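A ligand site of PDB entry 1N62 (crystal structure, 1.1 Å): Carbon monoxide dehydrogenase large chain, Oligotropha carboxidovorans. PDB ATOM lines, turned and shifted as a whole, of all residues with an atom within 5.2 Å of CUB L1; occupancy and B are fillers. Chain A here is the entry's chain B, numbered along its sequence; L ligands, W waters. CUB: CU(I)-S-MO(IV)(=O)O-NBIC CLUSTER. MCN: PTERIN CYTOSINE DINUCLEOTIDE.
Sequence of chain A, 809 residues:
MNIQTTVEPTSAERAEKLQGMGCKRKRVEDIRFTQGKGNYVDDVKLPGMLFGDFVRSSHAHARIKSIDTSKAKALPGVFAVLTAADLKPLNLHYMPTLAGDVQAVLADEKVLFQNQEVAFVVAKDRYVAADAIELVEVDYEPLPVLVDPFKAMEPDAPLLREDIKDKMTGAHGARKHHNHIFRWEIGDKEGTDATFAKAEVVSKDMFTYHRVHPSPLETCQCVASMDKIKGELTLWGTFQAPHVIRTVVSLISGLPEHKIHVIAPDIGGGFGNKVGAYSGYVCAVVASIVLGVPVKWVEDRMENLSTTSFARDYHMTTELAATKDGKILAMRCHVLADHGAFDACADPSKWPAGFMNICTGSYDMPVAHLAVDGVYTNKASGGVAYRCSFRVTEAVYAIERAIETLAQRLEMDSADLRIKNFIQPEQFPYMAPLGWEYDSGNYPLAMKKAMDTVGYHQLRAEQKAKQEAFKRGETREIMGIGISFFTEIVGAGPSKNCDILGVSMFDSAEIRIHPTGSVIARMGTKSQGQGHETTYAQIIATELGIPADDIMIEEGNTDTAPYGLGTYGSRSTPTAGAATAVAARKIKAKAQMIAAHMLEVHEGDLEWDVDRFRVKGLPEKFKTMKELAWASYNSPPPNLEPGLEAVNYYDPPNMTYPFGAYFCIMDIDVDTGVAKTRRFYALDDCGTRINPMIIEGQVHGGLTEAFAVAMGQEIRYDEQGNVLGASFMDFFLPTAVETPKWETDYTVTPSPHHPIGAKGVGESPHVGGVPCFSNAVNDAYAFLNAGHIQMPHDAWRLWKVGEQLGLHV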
ATOM      1  N   GLN A 240       1.149  19.130  18.995  1.00  0.00           N
ATOM      2  CA  GLN A 240       0.669  20.171  18.111  1.00  0.00           C
ATOM      3  C   GLN A 240       1.688  21.268  17.947  1.00  0.00           C
ATOM      4  O   GLN A 240       1.573  22.050  17.034  1.00  0.00           O
ATOM      5  CB  GLN A 240      -0.622  20.764  18.617  1.00  0.00           C
ATOM      6  CG  GLN A 240      -1.706  19.742  18.738  1.00  0.00           C
ATOM      7  CD  GLN A 240      -3.062  20.279  19.091  1.00  0.00           C
ATOM      8  OE1 GLN A 240      -3.809  19.608  19.780  1.00  0.00           O
ATOM      9  NE2 GLN A 240      -3.373  21.472  18.671  1.00  0.00           N
ATOM     10  N   PHE A 271      -7.134  18.584  18.125  1.00  0.00           N
ATOM     11  CA  PHE A 271      -8.274  19.337  18.621  1.00  0.00           C
ATOM     12  C   PHE A 271      -7.932  20.057  19.919  1.00  0.00           C
ATOM     13  O   PHE A 271      -8.805  20.329  20.704  1.00  0.00           O
ATOM     14  CB  PHE A 271      -9.481  18.446  18.773  1.00  0.00           C
ATOM     15  CG  PHE A 271      -9.758  17.614  17.594  1.00  0.00           C
ATOM     16  CD1 PHE A 271     -10.259  18.151  16.422  1.00  0.00           C
ATOM     17  CD2 PHE A 271      -9.441  16.282  17.618  1.00  0.00           C
ATOM     18  CE1 PHE A 271     -10.467  17.335  15.329  1.00  0.00           C
ATOM     19  CE2 PHE A 271      -9.660  15.494  16.538  1.00  0.00           C
ATOM     20  CZ  PHE A 271     -10.135  16.006  15.379  1.00  0.00           C
ATOM     21  N   GLY A 272      -6.668  20.391  20.113  1.00  0.00           N
ATOM     22  CA  GLY A 272      -6.201  21.113  21.264  1.00  0.00           C
ATOM     23  C   GLY A 272      -5.728  20.255  22.384  1.00  0.00           C
ATOM     24  O   GLY A 272      -5.127  20.740  23.337  1.00  0.00           O
ATOM     25  N   VAL A 275      -1.501  20.071  22.708  1.00  0.00           N
ATOM     26  CA  VAL A 275      -0.653  21.223  22.758  1.00  0.00           C
ATOM     27  C   VAL A 275       0.355  21.092  23.888  1.00  0.00           C
ATOM     28  O   VAL A 275       1.567  21.237  23.695  1.00  0.00           O
ATOM     29  CB  VAL A 275      -1.497  22.470  22.949  1.00  0.00           C
ATOM     30  CG1 VAL A 275      -0.578  23.630  23.072  1.00  0.00           C
ATOM     31  CG2 VAL A 275      -2.412  22.673  21.774  1.00  0.00           C
ATOM     32  N   ALA A 346      -3.856  26.202  28.617  1.00  0.00           N
ATOM     33  CA  ALA A 346      -3.059  26.734  27.565  1.00  0.00           C
ATOM     34  C   ALA A 346      -3.617  28.124  27.277  1.00  0.00           C
ATOM     35  O   ALA A 346      -4.819  28.404  27.328  1.00  0.00           O
ATOM     36  CB  ALA A 346      -3.149  25.878  26.335  1.00  0.00           C
ATOM     37  N   ASP A 347      -2.723  29.042  27.027  1.00  0.00           N
ATOM     38  CA  ASP A 347      -3.105  30.361  26.666  1.00  0.00           C
ATOM     39  C   ASP A 347      -1.809  31.052  26.396  1.00  0.00           C
ATOM     40  O   ASP A 347      -0.773  30.696  26.942  1.00  0.00           O
ATOM     41  CB  ASP A 347      -3.730  31.113  27.805  1.00  0.00           C
ATOM     42  CG  ASP A 347      -5.217  30.909  27.939  1.00  0.00           C
ATOM     43  OD1 ASP A 347      -5.947  31.071  26.965  1.00  0.00           O
ATOM     44  OD2 ASP A 347      -5.724  30.687  29.061  1.00  0.00           O
ATOM     45  N   VAL A 384      -8.492  25.248  27.986  1.00  0.00           N
ATOM     46  CA  VAL A 384      -8.371  25.655  26.621  1.00  0.00           C
ATOM     47  C   VAL A 384      -7.985  24.471  25.777  1.00  0.00           C
ATOM     48  O   VAL A 384      -6.893  23.902  25.909  1.00  0.00           O
ATOM     49  CB  VAL A 384      -7.374  26.792  26.546  1.00  0.00           C
ATOM     50  CG1 VAL A 384      -6.838  26.971  25.129  1.00  0.00           C
ATOM     51  CG2 VAL A 384      -8.050  28.047  27.024  1.00  0.00           C
ATOM     52  N   ALA A 385      -8.913  24.079  24.938  1.00  0.00           N
ATOM     53  CA  ALA A 385      -8.822  22.932  24.080  1.00  0.00           C
ATOM     54  C   ALA A 385     -10.124  22.854  23.326  1.00  0.00           C
ATOM     55  O   ALA A 385     -11.057  23.597  23.591  1.00  0.00           O
ATOM     56  CB  ALA A 385      -8.576  21.650  24.896  1.00  0.00           C
ATOM     57  N   TYR A 386     -10.186  21.965  22.355  1.00  0.00           N
ATOM     58  CA  TYR A 386     -11.418  21.590  21.711  1.00  0.00           C
ATOM     59  C   TYR A 386     -12.007  22.756  20.933  1.00  0.00           C
ATOM     60  O   TYR A 386     -13.148  23.140  21.120  1.00  0.00           O
ATOM     61  CB  TYR A 386     -12.380  21.042  22.724  1.00  0.00           C
ATOM     62  CG  TYR A 386     -13.456  20.169  22.228  1.00  0.00           C
ATOM     63  CD1 TYR A 386     -13.525  19.695  20.937  1.00  0.00           C
ATOM     64  CD2 TYR A 386     -14.395  19.735  23.115  1.00  0.00           C
ATOM     65  CE1 TYR A 386     -14.509  18.851  20.580  1.00  0.00           C
ATOM     66  CE2 TYR A 386     -15.357  18.857  22.749  1.00  0.00           C
ATOM     67  CZ  TYR A 386     -15.431  18.413  21.481  1.00  0.00           C
ATOM     68  OH  TYR A 386     -16.437  17.566  21.114  1.00  0.00           O
ATOM     69  N   ARG A 387     -11.225  23.261  20.001  1.00  0.00           N
ATOM     70  CA  ARG A 387     -11.642  24.316  19.100  1.00  0.00           C
ATOM     71  C   ARG A 387     -12.126  25.549  19.818  1.00  0.00           C
ATOM     72  O   ARG A 387     -13.023  26.232  19.326  1.00  0.00           O
ATOM     73  CB  ARG A 387     -12.682  23.820  18.109  1.00  0.00           C
ATOM     74  CG  ARG A 387     -12.205  22.709  17.246  1.00  0.00           C
ATOM     75  CD  ARG A 387     -12.969  22.548  15.953  1.00  0.00           C
ATOM     76  NE  ARG A 387     -12.739  21.200  15.407  1.00  0.00           N
ATOM     77  CZ  ARG A 387     -12.956  20.821  14.169  1.00  0.00           C
ATOM     78  NH1 ARG A 387     -13.066  21.690  13.180  1.00  0.00           N
ATOM     79  NH2 ARG A 387     -13.049  19.540  13.927  1.00  0.00           N
ATOM     80  N   CYS A 388     -11.466  25.904  20.921  1.00  0.00           N
ATOM     81  CA  CYS A 388     -11.914  27.071  21.663  1.00  0.00           C
ATOM     82  C   CYS A 388     -11.349  28.369  21.201  1.00  0.00           C
ATOM     83  O   CYS A 388     -11.841  29.427  21.632  1.00  0.00           O
ATOM     84  CB  CYS A 388     -11.788  26.881  23.139  1.00  0.00           C
ATOM     85  SG  CYS A 388     -10.211  27.131  23.935  1.00  0.00           S
ATOM     86  N   SER A 389     -10.227  28.341  20.510  1.00  0.00           N
ATOM     87  CA  SER A 389      -9.584  29.563  20.059  1.00  0.00           C
ATOM     88  C   SER A 389      -9.123  30.434  21.203  1.00  0.00           C
ATOM     89  O   SER A 389      -8.931  31.604  21.000  1.00  0.00           O
ATOM     90  CB  SER A 389     -10.445  30.369  19.101  1.00  0.00           C
ATOM     91  OG  SER A 389     -10.902  29.576  18.025  1.00  0.00           O
ATOM     92  N   PHE A 390      -8.902  29.857  22.362  1.00  0.00           N
ATOM     93  CA  PHE A 390      -8.589  30.549  23.624  1.00  0.00           C
ATOM     94  C   PHE A 390      -9.859  31.191  24.168  1.00  0.00           C
ATOM     95  O   PHE A 390     -10.003  32.389  24.260  1.00  0.00           O
ATOM     96  CB  PHE A 390      -7.495  31.586  23.494  1.00  0.00           C
ATOM     97  CG  PHE A 390      -6.207  31.064  22.991  1.00  0.00           C
ATOM     98  CD1 PHE A 390      -5.450  30.202  23.749  1.00  0.00           C
ATOM     99  CD2 PHE A 390      -5.683  31.555  21.816  1.00  0.00           C
ATOM    100  CE1 PHE A 390      -4.188  29.849  23.342  1.00  0.00           C
ATOM    101  CE2 PHE A 390      -4.491  31.095  21.327  1.00  0.00           C
ATOM    102  CZ  PHE A 390      -3.721  30.264  22.108  1.00  0.00           C
ATOM    103  N   ARG A 391     -10.789  30.346  24.570  1.00  0.00           N
ATOM    104  CA  ARG A 391     -12.000  30.764  25.267  1.00  0.00           C
ATOM    105  C   ARG A 391     -12.968  31.537  24.402  1.00  0.00           C
ATOM    106  O   ARG A 391     -13.917  32.154  24.897  1.00  0.00           O
ATOM    107  CB  ARG A 391     -11.713  31.518  26.534  1.00  0.00           C
ATOM    108  CG  ARG A 391     -10.862  30.834  27.503  1.00  0.00           C
ATOM    109  CD  ARG A 391     -11.483  29.547  28.009  1.00  0.00           C
ATOM    110  NE  ARG A 391     -10.724  29.029  29.127  1.00  0.00           N
ATOM    111  CZ  ARG A 391     -11.103  28.027  29.879  1.00  0.00           C
ATOM    112  NH1 ARG A 391     -12.208  27.395  29.575  1.00  0.00           N
ATOM    113  NH2 ARG A 391     -10.362  27.649  30.915  1.00  0.00           N
ATOM    114  N   GLN A 528      -2.685  18.176  12.407  1.00  0.00           N
ATOM    115  CA  GLN A 528      -3.240  16.963  12.933  1.00  0.00           C
ATOM    116  C   GLN A 528      -4.425  16.527  12.104  1.00  0.00           C
ATOM    117  O   GLN A 528      -5.409  16.022  12.628  1.00  0.00           O
ATOM    118  CB  GLN A 528      -3.602  17.108  14.395  1.00  0.00           C
ATOM    119  CG  GLN A 528      -2.587  17.838  15.222  1.00  0.00           C
ATOM    120  CD  GLN A 528      -3.095  19.167  15.681  1.00  0.00           C
ATOM    121  OE1 GLN A 528      -4.105  19.217  16.383  1.00  0.00           O
ATOM    122  NE2 GLN A 528      -2.455  20.231  15.304  1.00  0.00           N
ATOM    123  N   THR A 567       0.278  24.324  15.700  1.00  0.00           N
ATOM    124  CA  THR A 567      -1.082  24.433  15.224  1.00  0.00           C
ATOM    125  C   THR A 567      -2.068  24.327  16.337  1.00  0.00           C
ATOM    126  O   THR A 567      -2.190  23.262  16.919  1.00  0.00           O
ATOM    127  CB  THR A 567      -1.360  23.406  14.170  1.00  0.00           C
ATOM    128  OG1 THR A 567      -0.613  23.730  13.003  1.00  0.00           O
ATOM    129  CG2 THR A 567      -2.810  23.305  13.782  1.00  0.00           C
ATOM    130  N   TYR A 568      -2.755  25.417  16.564  1.00  0.00           N
ATOM    131  CA  TYR A 568      -3.865  25.559  17.490  1.00  0.00           C
ATOM    132  C   TYR A 568      -4.379  26.937  17.259  1.00  0.00           C
ATOM    133  O   TYR A 568      -3.839  27.690  16.459  1.00  0.00           O
ATOM    134  CB  TYR A 568      -3.441  25.329  18.932  1.00  0.00           C
ATOM    135  CG  TYR A 568      -2.220  26.062  19.339  1.00  0.00           C
ATOM    136  CD1 TYR A 568      -2.243  27.423  19.509  1.00  0.00           C
ATOM    137  CD2 TYR A 568      -1.000  25.424  19.414  1.00  0.00           C
ATOM    138  CE1 TYR A 568      -1.106  28.119  19.842  1.00  0.00           C
ATOM    139  CE2 TYR A 568       0.134  26.103  19.741  1.00  0.00           C
ATOM    140  CZ  TYR A 568       0.076  27.461  19.909  1.00  0.00           C
ATOM    141  OH  TYR A 568       1.216  28.171  20.156  1.00  0.00           O
ATOM    142  N   GLY A 569      -5.503  27.271  17.845  1.00  0.00           N
ATOM    143  CA  GLY A 569      -6.084  28.559  17.657  1.00  0.00           C
ATOM    144  C   GLY A 569      -6.417  28.931  16.244  1.00  0.00           C
ATOM    145  O   GLY A 569      -6.394  30.106  15.918  1.00  0.00           O
ATOM    146  N   SER A 570      -6.630  27.941  15.381  1.00  0.00           N
ATOM    147  CA  SER A 570      -6.872  28.182  13.991  1.00  0.00           C
ATOM    148  C   SER A 570      -5.854  29.096  13.442  1.00  0.00           C
ATOM    149  O   SER A 570      -6.131  29.897  12.554  1.00  0.00           O
ATOM    150  CB  SER A 570      -8.248  28.719  13.695  1.00  0.00           C
ATOM    151  OG  SER A 570      -9.220  27.929  14.303  1.00  0.00           O
ATOM    152  N   GLU A 763     -11.656  26.349  13.810  1.00  0.00           N
ATOM    153  CA  GLU A 763     -12.414  26.315  15.045  1.00  0.00           C
ATOM    154  C   GLU A 763     -13.775  26.976  14.933  1.00  0.00           C
ATOM    155  O   GLU A 763     -14.627  26.719  15.763  1.00  0.00           O
ATOM    156  CB  GLU A 763     -11.646  26.932  16.147  1.00  0.00           C
ATOM    157  CG  GLU A 763     -10.384  26.162  16.466  1.00  0.00           C
ATOM    158  CD  GLU A 763      -9.548  26.917  17.423  1.00  0.00           C
ATOM    159  OE1 GLU A 763      -9.122  28.020  17.040  1.00  0.00           O
ATOM    160  OE2 GLU A 763      -9.362  26.529  18.585  1.00  0.00           O
HETATM  161  C3Z CUB L   1      -4.566  26.568  22.556  1.00  0.00           C
HETATM  162  C2Z CUB L   1      -5.015  27.253  21.471  1.00  0.00           C
HETATM  163  C1Z CUB L   1      -6.353  27.651  21.422  1.00  0.00           C
HETATM  164  NZ  CUB L   1      -7.220  26.520  21.641  1.00  0.00           N
HETATM  165 CU   CUB L   1      -8.658  26.626  22.760  1.00  0.00          CU
HETATM  166 MO   CUB L   1      -7.167  23.917  18.727  1.00  0.00          MO
HETATM  167  S   CUB L   1      -8.202  24.202  20.825  1.00  0.00           S
HETATM  168  CZ  CUB L   1      -7.288  25.644  20.660  1.00  0.00           C
HETATM  169  OM2 CUB L   1      -6.658  25.652  19.554  1.00  0.00           O
HETATM  170  C4Z CUB L   1      -2.977  26.420  22.780  1.00  0.00           C
HETATM  171  OM1 CUB L   1      -5.803  22.959  18.800  1.00  0.00           O
HETATM  172  N1  MCN L   2      -8.199  26.885   5.055  1.00  0.00           N
HETATM  173  C2  MCN L   2      -8.489  27.348   3.826  1.00  0.00           C
HETATM  174  N3  MCN L   2      -8.762  28.655   3.695  1.00  0.00           N
HETATM  175  C4  MCN L   2      -8.855  29.433   4.754  1.00  0.00           C
HETATM  176  C5  MCN L   2      -8.663  28.923   6.062  1.00  0.00           C
HETATM  177  C6  MCN L   2      -8.309  27.680   6.169  1.00  0.00           C
HETATM  178  O2  MCN L   2      -8.557  26.602   2.860  1.00  0.00           O
HETATM  179  N4  MCN L   2      -9.021  30.750   4.675  1.00  0.00           N
HETATM  180  C1' MCN L   2      -7.642  25.532   5.196  1.00  0.00           C
HETATM  181  C2D MCN L   2      -6.180  25.615   5.616  1.00  0.00           C
HETATM  182  O2' MCN L   2      -5.379  25.769   4.478  1.00  0.00           O
HETATM  183  C3' MCN L   2      -5.958  24.368   6.370  1.00  0.00           C
HETATM  184  C4D MCN L   2      -7.328  24.187   7.032  1.00  0.00           C
HETATM  185  O4D MCN L   2      -8.286  24.901   6.217  1.00  0.00           O
HETATM  186  O3' MCN L   2      -5.649  23.320   5.458  1.00  0.00           O
HETATM  187  C5' MCN L   2      -7.418  24.673   8.429  1.00  0.00           C
HETATM  188  O5' MCN L   2      -6.700  25.901   8.546  1.00  0.00           O
HETATM  189  PA  MCN L   2      -6.835  26.877   9.800  1.00  0.00           P
HETATM  190  O1A MCN L   2      -5.728  27.826   9.628  1.00  0.00           O
HETATM  191  O2A MCN L   2      -8.204  27.355   9.898  1.00  0.00           O
HETATM  192  O3A MCN L   2      -6.602  25.960  11.064  1.00  0.00           O
HETATM  193  PB  MCN L   2      -5.347  25.129  11.526  1.00  0.00           P
HETATM  194  O1B MCN L   2      -4.504  25.982  12.357  1.00  0.00           O
HETATM  195  O2B MCN L   2      -4.775  24.447  10.349  1.00  0.00           O
HETATM  196  O3B MCN L   2      -6.022  24.028  12.355  1.00  0.00           O
HETATM  197  C10 MCN L   2      -6.265  24.183  13.767  1.00  0.00           C
HETATM  198  C9' MCN L   2      -7.716  23.903  14.044  1.00  0.00           C
HETATM  199  C8' MCN L   2      -7.960  23.759  15.479  1.00  0.00           C
HETATM  200  S8' MCN L   2      -7.125  24.890  16.567  1.00  0.00           S
HETATM  201  C7' MCN L   2      -8.668  22.768  15.969  1.00  0.00           C
HETATM  202  S7' MCN L   2      -8.746  22.567  17.760  1.00  0.00           S
HETATM  203  C6' MCN L   2      -9.043  21.706  15.227  1.00  0.00           C
HETATM  204  C7  MCN L   2      -9.298  22.176  13.774  1.00  0.00           C
HETATM  205  O9' MCN L   2      -8.061  22.706  13.364  1.00  0.00           O
HETATM  206  N5' MCN L   2      -8.322  20.548  15.250  1.00  0.00           N
HETATM  207  C4A MCN L   2      -8.356  19.669  14.190  1.00  0.00           C
HETATM  208  N8' MCN L   2      -9.638  21.153  12.864  1.00  0.00           N
HETATM  209  C4B MCN L   2      -9.051  19.958  13.057  1.00  0.00           C
HETATM  210  N1' MCN L   2      -9.237  19.066  12.045  1.00  0.00           N
HETATM  211  C2' MCN L   2      -8.578  17.918  12.104  1.00  0.00           C
HETATM  212  N2' MCN L   2      -8.664  16.997  11.117  1.00  0.00           N
HETATM  213  N3' MCN L   2      -7.794  17.655  13.155  1.00  0.00           N
HETATM  214  C4' MCN L   2      -7.661  18.463  14.260  1.00  0.00           C
HETATM  215  O4' MCN L   2      -6.932  18.139  15.189  1.00  0.00           O
HETATM  216  O   HOH W   1      -5.492  21.514  16.046  1.00  0.00           O
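Water W1 lies within hydrogen-bond range of the side-chain amide oxygen (OE1) of Gln 528 (2.7 Å), a nitrogen (N5') of MCN L2 (3.1 Å) and the side-chain amide nitrogen (NE2) of Gln 240 (3.4 Å).
S of CUB L1 sits close to N of Cys 388. A copper atom (CU) of CUB L1 is bound by the side-chain sulfur (SG) of Cys 388 (2.0 Å). The backbone NH (N) of Gly 569 sits close to an oxygen (OM2) of CUB L1, at 2.6 Å. The backbone NH (N) of Arg 387 sits close to a sulfur (S) of CUB L1 (3.3 Å). The backbone NH of Tyr 386 lies close to a sulfur (S) of CUB L1 (3.4 Å). The backbone NH (N) of Gly 569 lies close to a sulfur (S8') of MCN L2 (3.2 Å). S8' of MCN L2 lies close to OE2 of Glu 763, at 3.4 Å. N of Arg 387 lies close to S7' of MCN L2, 3.4 Å away. NH1 of Arg 387 is in hydrogen-bond range of N8' of MCN L2 (3.5 Å). The backbone NH (N) of Phe 271 sits at hydrogen-bond distance from an oxygen (O4') of MCN L2, at 3.0 Å. S7' of MCN L2 sits close to O of Phe 271, 3.7 Å away. A sulfur (S8') of MCN L2 lies close to the backbone NH (N) of Ser 570, at 3.3 Å. An oxygen (O4') of MCN L2 sits at hydrogen-bond distance from the side-chain amide oxygen of Gln 528, at 3.3 Å.
OE2 of Glu 763 lies within hydrogen-bond range of N of Cys 388. N of Arg 391 lies close to SG of Cys 388 (3.3 Å). The side-chain amide oxygen (OE1) of Gln 240 is in hydrogen-bond range of the backbone NH (N) of Gly 272, at 3.0 Å. The side-chain amide nitrogen of Gln 240 lies within hydrogen-bond range of the backbone carbonyl oxygen of Thr 567 (2.8 Å). The side-chain amide nitrogen (NE2) of Gln 240 lies close to the side-chain amide oxygen (OE1) of Gln 528, 3.3 Å away. OE1 of Glu 763 is in hydrogen-bond range of OG of Ser 389 (2.6 Å). The side-chain hydroxyl (OG) of Ser 570 lies within hydrogen-bond range of the side-chain carboxylate (OE1) of Glu 763, at 2.7 Å. The backbone NH (N) of Tyr 386 is in hydrogen-bond range of the backbone carbonyl oxygen (O) of Phe 271, at 2.7 Å.
MO of CUB L1 is bound by S7' of MCN L2, 2.3 Å away.
NE2 of Gln 240 lies close to OM1 of CUB L1 (2.9 Å). The backbone NH (N) of Gly 272 lies close to an oxygen (OM1) of CUB L1. The side-chain carboxylate of Glu 763 lies close to an oxygen (OM2) of CUB L1 (3.0 Å). Residues that only touch CUB L1: Val 384 (3.0 Å), Ser 389 (3.2 Å), Phe 390 (3.3 Å), Tyr 568 (3.3 Å), Ala 385 (3.4 Å), Ala 346 (3.6 Å), Val 275 (3.7 Å) and Phe 271 (3.8 Å). Hydrophobic or aromatic side chains within 4 Å of CUB L1: Val 275, Ala 346, Val 384, Phe 390 and Tyr 568. Within 4 Å of CUB L1: Gln 240, Phe 271, Gly 272, Val 275, Ala 346, Val 384, Ala 385, Tyr 386, Arg 387, Cys 388, Ser 389, Phe 390, Tyr 568, Gly 569 and Glu 763. The nearest printed residue that does not touch CUB L1 is Thr 567 (4.1 Å).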
